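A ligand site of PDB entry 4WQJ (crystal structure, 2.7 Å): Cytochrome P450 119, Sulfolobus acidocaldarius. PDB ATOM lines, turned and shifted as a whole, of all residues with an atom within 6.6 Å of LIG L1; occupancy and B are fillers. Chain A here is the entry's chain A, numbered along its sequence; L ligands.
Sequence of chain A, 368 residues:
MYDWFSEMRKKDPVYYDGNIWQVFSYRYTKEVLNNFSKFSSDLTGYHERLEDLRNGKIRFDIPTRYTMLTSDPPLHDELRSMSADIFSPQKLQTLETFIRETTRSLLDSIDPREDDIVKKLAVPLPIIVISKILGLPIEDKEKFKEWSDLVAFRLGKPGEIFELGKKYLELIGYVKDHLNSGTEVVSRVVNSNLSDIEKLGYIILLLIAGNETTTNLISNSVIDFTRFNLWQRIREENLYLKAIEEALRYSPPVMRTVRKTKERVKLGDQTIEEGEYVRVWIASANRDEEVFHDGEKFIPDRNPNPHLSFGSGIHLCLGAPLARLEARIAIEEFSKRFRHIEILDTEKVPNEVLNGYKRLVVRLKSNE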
ATOM      1  N   LEU A  69      -9.357  -8.901  31.251  1.00  0.00           N
ATOM      2  CA  LEU A  69      -8.720  -8.552  29.982  1.00  0.00           C
ATOM      3  C   LEU A  69      -9.760  -8.158  28.957  1.00  0.00           C
ATOM      4  O   LEU A  69      -9.505  -7.326  28.087  1.00  0.00           O
ATOM      5  CB  LEU A  69      -7.870  -9.717  29.475  1.00  0.00           C
ATOM      6  CG  LEU A  69      -7.118  -9.527  28.156  1.00  0.00           C
ATOM      7  CD1 LEU A  69      -6.004  -8.460  28.241  1.00  0.00           C
ATOM      8  CD2 LEU A  69      -6.563 -10.857  27.742  1.00  0.00           C
ATOM      9  N   VAL A 151      -1.773 -20.740  25.352  1.00  0.00           N
ATOM     10  CA  VAL A 151      -1.991 -19.326  25.104  1.00  0.00           C
ATOM     11  C   VAL A 151      -1.616 -19.040  23.655  1.00  0.00           C
ATOM     12  O   VAL A 151      -0.563 -19.479  23.196  1.00  0.00           O
ATOM     13  CB  VAL A 151      -1.184 -18.449  26.116  1.00  0.00           C
ATOM     14  CG1 VAL A 151       0.239 -18.165  25.634  1.00  0.00           C
ATOM     15  CG2 VAL A 151      -1.896 -17.156  26.386  1.00  0.00           C
ATOM     16  N   ALA A 152      -2.482 -18.368  22.907  1.00  0.00           N
ATOM     17  CA  ALA A 152      -2.316 -18.241  21.454  1.00  0.00           C
ATOM     18  C   ALA A 152      -3.375 -17.348  20.796  1.00  0.00           C
ATOM     19  O   ALA A 152      -4.502 -17.271  21.275  1.00  0.00           O
ATOM     20  CB  ALA A 152      -2.358 -19.618  20.796  1.00  0.00           C
ATOM     21  N   PHE A 153      -3.011 -16.684  19.702  1.00  0.00           N
ATOM     22  CA  PHE A 153      -4.000 -16.032  18.860  1.00  0.00           C
ATOM     23  C   PHE A 153      -4.876 -17.094  18.214  1.00  0.00           C
ATOM     24  O   PHE A 153      -4.383 -17.969  17.524  1.00  0.00           O
ATOM     25  CB  PHE A 153      -3.361 -15.161  17.778  1.00  0.00           C
ATOM     26  CG  PHE A 153      -4.344 -14.649  16.736  1.00  0.00           C
ATOM     27  CD1 PHE A 153      -5.251 -13.622  17.051  1.00  0.00           C
ATOM     28  CD2 PHE A 153      -4.372 -15.185  15.447  1.00  0.00           C
ATOM     29  CE1 PHE A 153      -6.164 -13.137  16.100  1.00  0.00           C
ATOM     30  CE2 PHE A 153      -5.292 -14.712  14.479  1.00  0.00           C
ATOM     31  CZ  PHE A 153      -6.182 -13.682  14.807  1.00  0.00           C
ATOM     32  N   ARG A 154      -6.177 -16.990  18.438  1.00  0.00           N
ATOM     33  CA  ARG A 154      -7.138 -17.881  17.792  1.00  0.00           C
ATOM     34  C   ARG A 154      -7.807 -17.079  16.679  1.00  0.00           C
ATOM     35  O   ARG A 154      -8.366 -16.019  16.934  1.00  0.00           O
ATOM     36  CB  ARG A 154      -8.178 -18.404  18.795  1.00  0.00           C
ATOM     37  CG  ARG A 154      -7.628 -18.898  20.144  1.00  0.00           C
ATOM     38  CD  ARG A 154      -7.159 -20.353  20.097  1.00  0.00           C
ATOM     39  NE  ARG A 154      -8.143 -21.284  19.511  1.00  0.00           N
ATOM     40  CZ  ARG A 154      -9.323 -21.605  20.047  1.00  0.00           C
ATOM     41  NH1 ARG A 154      -9.727 -21.061  21.186  1.00  0.00           N
ATOM     42  NH2 ARG A 154     -10.125 -22.474  19.433  1.00  0.00           N
ATOM     43  N   GLU A 160     -10.357 -14.287  22.567  1.00  0.00           N
ATOM     44  CA  GLU A 160      -9.992 -15.599  23.090  1.00  0.00           C
ATOM     45  C   GLU A 160      -8.490 -15.867  22.898  1.00  0.00           C
ATOM     46  O   GLU A 160      -8.011 -15.846  21.762  1.00  0.00           O
ATOM     47  CB  GLU A 160     -10.807 -16.714  22.420  1.00  0.00           C
ATOM     48  CG  GLU A 160     -12.287 -16.730  22.755  1.00  0.00           C
ATOM     49  CD  GLU A 160     -12.813 -18.141  22.970  1.00  0.00           C
ATOM     50  OE1 GLU A 160     -11.997 -19.027  23.342  1.00  0.00           O
ATOM     51  OE2 GLU A 160     -14.043 -18.350  22.770  1.00  0.00           O
ATOM     52  N   ILE A 161      -7.765 -16.098  23.978  1.00  0.00           N
ATOM     53  CA  ILE A 161      -6.330 -16.371  23.875  1.00  0.00           C
ATOM     54  C   ILE A 161      -5.924 -17.758  24.397  1.00  0.00           C
ATOM     55  O   ILE A 161      -4.749 -18.063  24.556  1.00  0.00           O
ATOM     56  CB  ILE A 161      -5.483 -15.300  24.601  1.00  0.00           C
ATOM     57  CG1 ILE A 161      -5.792 -15.302  26.110  1.00  0.00           C
ATOM     58  CG2 ILE A 161      -5.683 -13.932  23.948  1.00  0.00           C
ATOM     59  CD1 ILE A 161      -4.694 -14.676  26.975  1.00  0.00           C
ATOM     60  N   LEU A 205      -6.110 -16.914  34.252  1.00  0.00           N
ATOM     61  CA  LEU A 205      -5.503 -15.752  33.645  1.00  0.00           C
ATOM     62  C   LEU A 205      -4.180 -15.388  34.341  1.00  0.00           C
ATOM     63  O   LEU A 205      -3.150 -15.294  33.679  1.00  0.00           O
ATOM     64  CB  LEU A 205      -6.454 -14.581  33.698  1.00  0.00           C
ATOM     65  CG  LEU A 205      -5.820 -13.380  32.997  1.00  0.00           C
ATOM     66  CD1 LEU A 205      -5.631 -13.704  31.536  1.00  0.00           C
ATOM     67  CD2 LEU A 205      -6.618 -12.112  33.177  1.00  0.00           C
ATOM     68  N   ILE A 208      -1.423 -18.403  34.075  1.00  0.00           N
ATOM     69  CA  ILE A 208      -0.926 -18.891  32.795  1.00  0.00           C
ATOM     70  C   ILE A 208      -0.543 -17.786  31.812  1.00  0.00           C
ATOM     71  O   ILE A 208       0.534 -17.813  31.241  1.00  0.00           O
ATOM     72  CB  ILE A 208      -1.981 -19.824  32.154  1.00  0.00           C
ATOM     73  CG1 ILE A 208      -2.221 -21.046  33.059  1.00  0.00           C
ATOM     74  CG2 ILE A 208      -1.584 -20.268  30.796  1.00  0.00           C
ATOM     75  CD1 ILE A 208      -0.966 -21.773  33.470  1.00  0.00           C
ATOM     76  N   ALA A 209      -1.422 -16.807  31.651  1.00  0.00           N
ATOM     77  CA  ALA A 209      -1.311 -15.831  30.589  1.00  0.00           C
ATOM     78  C   ALA A 209       0.028 -15.127  30.482  1.00  0.00           C
ATOM     79  O   ALA A 209       0.424 -14.741  29.392  1.00  0.00           O
ATOM     80  CB  ALA A 209      -2.388 -14.803  30.740  1.00  0.00           C
ATOM     81  N   GLY A 210       0.728 -14.956  31.599  1.00  0.00           N
ATOM     82  CA  GLY A 210       1.974 -14.200  31.565  1.00  0.00           C
ATOM     83  C   GLY A 210       3.268 -14.988  31.406  1.00  0.00           C
ATOM     84  O   GLY A 210       4.361 -14.405  31.341  1.00  0.00           O
ATOM     85  N   ASN A 211       3.162 -16.318  31.332  1.00  0.00           N
ATOM     86  CA  ASN A 211       4.365 -17.143  31.277  1.00  0.00           C
ATOM     87  C   ASN A 211       5.141 -17.031  29.966  1.00  0.00           C
ATOM     88  O   ASN A 211       6.243 -16.486  29.935  1.00  0.00           O
ATOM     89  CB  ASN A 211       3.969 -18.585  31.544  1.00  0.00           C
ATOM     90  CG  ASN A 211       3.461 -18.750  32.933  1.00  0.00           C
ATOM     91  OD1 ASN A 211       3.742 -17.908  33.800  1.00  0.00           O
ATOM     92  ND2 ASN A 211       2.701 -19.817  33.179  1.00  0.00           N
ATOM     93  N   THR A 213       4.883 -15.005  27.520  1.00  0.00           N
ATOM     94  CA  THR A 213       5.283 -13.626  27.179  1.00  0.00           C
ATOM     95  C   THR A 213       6.577 -13.213  27.895  1.00  0.00           C
ATOM     96  O   THR A 213       7.410 -12.475  27.336  1.00  0.00           O
ATOM     97  CB  THR A 213       4.172 -12.593  27.536  1.00  0.00           C
ATOM     98  OG1 THR A 213       3.668 -12.852  28.843  1.00  0.00           O
ATOM     99  CG2 THR A 213       3.025 -12.625  26.541  1.00  0.00           C
ATOM    100  N   VAL A 254       4.532  -9.248  22.789  1.00  0.00           N
ATOM    101  CA  VAL A 254       3.195  -9.166  22.185  1.00  0.00           C
ATOM    102  C   VAL A 254       3.220  -8.112  21.079  1.00  0.00           C
ATOM    103  O   VAL A 254       3.602  -6.971  21.330  1.00  0.00           O
ATOM    104  CB  VAL A 254       2.124  -8.833  23.245  1.00  0.00           C
ATOM    105  CG1 VAL A 254       0.745  -8.728  22.604  1.00  0.00           C
ATOM    106  CG2 VAL A 254       2.140  -9.881  24.342  1.00  0.00           C
ATOM    107  N   ARG A 256       0.722  -7.114  18.840  1.00  0.00           N
ATOM    108  CA  ARG A 256      -0.485  -6.418  18.498  1.00  0.00           C
ATOM    109  C   ARG A 256      -1.560  -6.805  19.481  1.00  0.00           C
ATOM    110  O   ARG A 256      -1.428  -7.828  20.163  1.00  0.00           O
ATOM    111  CB  ARG A 256      -0.907  -6.759  17.066  1.00  0.00           C
ATOM    112  CG  ARG A 256      -1.603  -8.096  16.954  1.00  0.00           C
ATOM    113  CD  ARG A 256      -1.761  -8.464  15.508  1.00  0.00           C
ATOM    114  NE  ARG A 256      -2.699  -9.561  15.364  1.00  0.00           N
ATOM    115  CZ  ARG A 256      -2.574 -10.544  14.473  1.00  0.00           C
ATOM    116  NH1 ARG A 256      -1.534 -10.547  13.650  1.00  0.00           N
ATOM    117  NH2 ARG A 256      -3.480 -11.512  14.422  1.00  0.00           N
ATOM    118  N   THR A 257      -2.614  -5.990  19.544  1.00  0.00           N
ATOM    119  CA  THR A 257      -3.780  -6.328  20.331  1.00  0.00           C
ATOM    120  C   THR A 257      -4.976  -5.760  19.574  1.00  0.00           C
ATOM    121  O   THR A 257      -4.791  -5.179  18.508  1.00  0.00           O
ATOM    122  CB  THR A 257      -3.672  -5.786  21.759  1.00  0.00           C
ATOM    123  OG1 THR A 257      -4.739  -6.302  22.551  1.00  0.00           O
ATOM    124  CG2 THR A 257      -3.729  -4.278  21.769  1.00  0.00           C
ATOM    125  N   CYS A 317      -0.396  -3.594  31.387  1.00  0.00           N
ATOM    126  CA  CYS A 317      -0.163  -4.934  31.886  1.00  0.00           C
ATOM    127  C   CYS A 317       0.003  -5.016  33.410  1.00  0.00           C
ATOM    128  O   CYS A 317       0.987  -4.539  33.989  1.00  0.00           O
ATOM    129  CB  CYS A 317       1.076  -5.541  31.200  1.00  0.00           C
ATOM    130  SG  CYS A 317       1.434  -7.248  31.713  1.00  0.00           S
ATOM    131  N   GLY A 319       1.019  -7.375  35.025  1.00  0.00           N
ATOM    132  CA  GLY A 319       2.264  -8.057  35.336  1.00  0.00           C
ATOM    133  C   GLY A 319       3.520  -7.318  34.909  1.00  0.00           C
ATOM    134  O   GLY A 319       4.612  -7.880  34.979  1.00  0.00           O
ATOM    135  N   VAL A 353       1.048 -13.326  16.898  1.00  0.00           N
ATOM    136  CA  VAL A 353       0.905 -12.281  17.880  1.00  0.00           C
ATOM    137  C   VAL A 353       2.062 -12.359  18.871  1.00  0.00           C
ATOM    138  O   VAL A 353       2.607 -11.341  19.290  1.00  0.00           O
ATOM    139  CB  VAL A 353      -0.458 -12.384  18.614  1.00  0.00           C
ATOM    140  CG1 VAL A 353      -0.529 -11.422  19.794  1.00  0.00           C
ATOM    141  CG2 VAL A 353      -1.603 -12.092  17.651  1.00  0.00           C
ATOM    142  N   LEU A 354       2.440 -13.587  19.211  1.00  0.00           N
ATOM    143  CA  LEU A 354       3.524 -13.827  20.154  1.00  0.00           C
ATOM    144  C   LEU A 354       4.847 -13.900  19.436  1.00  0.00           C
ATOM    145  O   LEU A 354       4.973 -14.536  18.395  1.00  0.00           O
ATOM    146  CB  LEU A 354       3.271 -15.118  20.905  1.00  0.00           C
ATOM    147  CG  LEU A 354       2.017 -14.991  21.751  1.00  0.00           C
ATOM    148  CD1 LEU A 354       1.469 -16.349  22.071  1.00  0.00           C
ATOM    149  CD2 LEU A 354       2.406 -14.248  23.000  1.00  0.00           C
HETATM  150  C1  LIG L   1       0.233 -11.525  29.639  1.00  0.00           C
HETATM  151  C2  LIG L   1      -0.427 -10.200  28.020  1.00  0.00           C
HETATM  152  C3  LIG L   1      -0.586 -11.522  27.591  1.00  0.00           C
HETATM  153  C4  LIG L   1      -1.082 -12.030  26.246  1.00  0.00           C
HETATM  154  C5  LIG L   1      -1.675 -11.191  25.293  1.00  0.00           C
HETATM  155  C6  LIG L   1      -2.095 -11.705  24.056  1.00  0.00           C
HETATM  156  C7  LIG L   1      -1.917 -13.058  23.759  1.00  0.00           C
HETATM  157  C8  LIG L   1      -1.305 -13.895  24.703  1.00  0.00           C
HETATM  158 BR1  LIG L   1      -2.472 -13.822  22.079  1.00  0.00          BR
HETATM  159  C9  LIG L   1      -0.890 -13.382  25.931  1.00  0.00           C
HETATM  160  N1  LIG L   1      -0.151 -12.287  28.624  1.00  0.00           N
HETATM  161  N2  LIG L   1       0.072 -10.259  29.291  1.00  0.00           N
HETATM  162  C1  LG2 L   2      -2.257  -6.946  29.788  1.00  0.00           C
HETATM  163  C2  LG2 L   2       2.019  -7.512  27.546  1.00  0.00           C
HETATM  164  C3  LG2 L   2       3.672 -10.210  31.222  1.00  0.00           C
HETATM  165  C4  LG2 L   2      -0.827 -10.331  32.976  1.00  0.00           C
HETATM  166  C5  LG2 L   2      -1.244  -6.846  28.866  1.00  0.00           C
HETATM  167  C6  LG2 L   2      -1.273  -6.067  27.637  1.00  0.00           C
HETATM  168  C7  LG2 L   2      -0.087  -6.234  27.028  1.00  0.00           C
HETATM  169  C8  LG2 L   2       0.733  -7.110  27.843  1.00  0.00           C
HETATM  170  C9  LG2 L   2       0.365  -5.609  25.696  1.00  0.00           C
HETATM  171  C10 LG2 L   2      -2.445  -5.203  27.127  1.00  0.00           C
HETATM  172  C11 LG2 L   2      -3.639  -6.015  26.640  1.00  0.00           C
HETATM  173  C12 LG2 L   2      -4.594  -5.082  25.907  1.00  0.00           C
HETATM  174  O1  LG2 L   2      -4.635  -3.851  26.229  1.00  0.00           O
HETATM  175  O2  LG2 L   2      -5.320  -5.580  25.005  1.00  0.00           O
HETATM  176  C13 LG2 L   2       2.851  -8.235  28.372  1.00  0.00           C
HETATM  177  C14 LG2 L   2       4.277  -8.442  28.176  1.00  0.00           C
HETATM  178  C15 LG2 L   2       4.713  -9.218  29.187  1.00  0.00           C
HETATM  179  C16 LG2 L   2       3.595  -9.485  30.066  1.00  0.00           C
HETATM  180  C17 LG2 L   2       5.088  -7.877  26.967  1.00  0.00           C
HETATM  181  C18 LG2 L   2       6.132  -9.747  29.498  1.00  0.00           C
HETATM  182  C19 LG2 L   2       7.230  -9.309  28.889  1.00  0.00           C
HETATM  183  C20 LG2 L   2       2.609 -10.442  32.059  1.00  0.00           C
HETATM  184  C21 LG2 L   2       2.619 -11.119  33.342  1.00  0.00           C
HETATM  185  C22 LG2 L   2       1.353 -11.122  33.796  1.00  0.00           C
HETATM  186  C23 LG2 L   2       0.524 -10.476  32.821  1.00  0.00           C
HETATM  187  C24 LG2 L   2       3.865 -11.692  34.064  1.00  0.00           C
HETATM  188  C25 LG2 L   2       0.696 -11.695  35.065  1.00  0.00           C
HETATM  189  C26 LG2 L   2       1.228 -12.641  35.825  1.00  0.00           C
HETATM  190  C27 LG2 L   2      -1.616  -9.423  32.321  1.00  0.00           C
HETATM  191  C28 LG2 L   2      -2.979  -9.160  32.681  1.00  0.00           C
HETATM  192  C29 LG2 L   2      -3.435  -8.093  31.693  1.00  0.00           C
HETATM  193  C30 LG2 L   2      -2.298  -7.843  30.829  1.00  0.00           C
HETATM  194  C31 LG2 L   2      -3.805  -9.780  33.825  1.00  0.00           C
HETATM  195  C32 LG2 L   2      -4.810  -7.435  31.660  1.00  0.00           C
HETATM  196  C33 LG2 L   2      -4.810  -6.318  32.699  1.00  0.00           C
HETATM  197  C34 LG2 L   2      -6.070  -5.501  32.504  1.00  0.00           C
HETATM  198  O3  LG2 L   2      -6.851  -5.817  31.554  1.00  0.00           O
HETATM  199  O4  LG2 L   2      -6.291  -4.535  33.287  1.00  0.00           O
HETATM  200  N1  LG2 L   2       0.000  -7.468  28.959  1.00  0.00           N
HETATM  201  N2  LG2 L   2       2.471  -8.888  29.528  1.00  0.00           N
HETATM  202  N3  LG2 L   2       1.305 -10.079  31.767  1.00  0.00           N
HETATM  203  N4  LG2 L   2      -1.249  -8.647  31.236  1.00  0.00           N
HETATM  204 FE1  LG2 L   2       0.587  -8.842  30.374  1.00  0.00          FE
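An oxygen (O2) of LG2 L2 lies within hydrogen-bond range of the side-chain hydroxyl of Thr 257 (2.6 Å).
SG of Cys 317 binds FE1 of LG2 L2, 2.2 Å away.
A nitrogen (N1) of LIG L1 sits close to the backbone carbonyl oxygen of Ala 209, at 2.6 Å.
A nitrogen (N2) of LIG L1 is bound to an iron atom (FE1) of LG2 L2, at 1.9 Å.
The backbone carbonyl oxygen (O) of Gly 210 is in hydrogen-bond range of the side-chain hydroxyl (OG1) of Thr 213, at 3.0 Å.
The backbone carbonyl oxygen of Ile 161 lies within hydrogen-bond range of the backbone NH of Ala 152.
Val 151 touches LIG L1 (CG2 to C8, 3.7 Å).
Ala 152 touches LIG L1 (C to BR1, 3.9 Å).
Phe 153 touches LIG L1.
CG2 of Ile 161 touches BR1 of LIG L1, at 3.7 Å.
Gly 210 touches LIG L1.
Thr 213 touches LIG L1 (OG1 to C1, 3.8 Å).
Val 353 touches LIG L1.
Hydrophobic or aromatic side chains within 4 Å of LIG L1: Val 151, Ile 161, Ala 209 and Val 353.
The nearest printed residue that does not touch LIG L1 is Cys 317 (4.1 Å).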
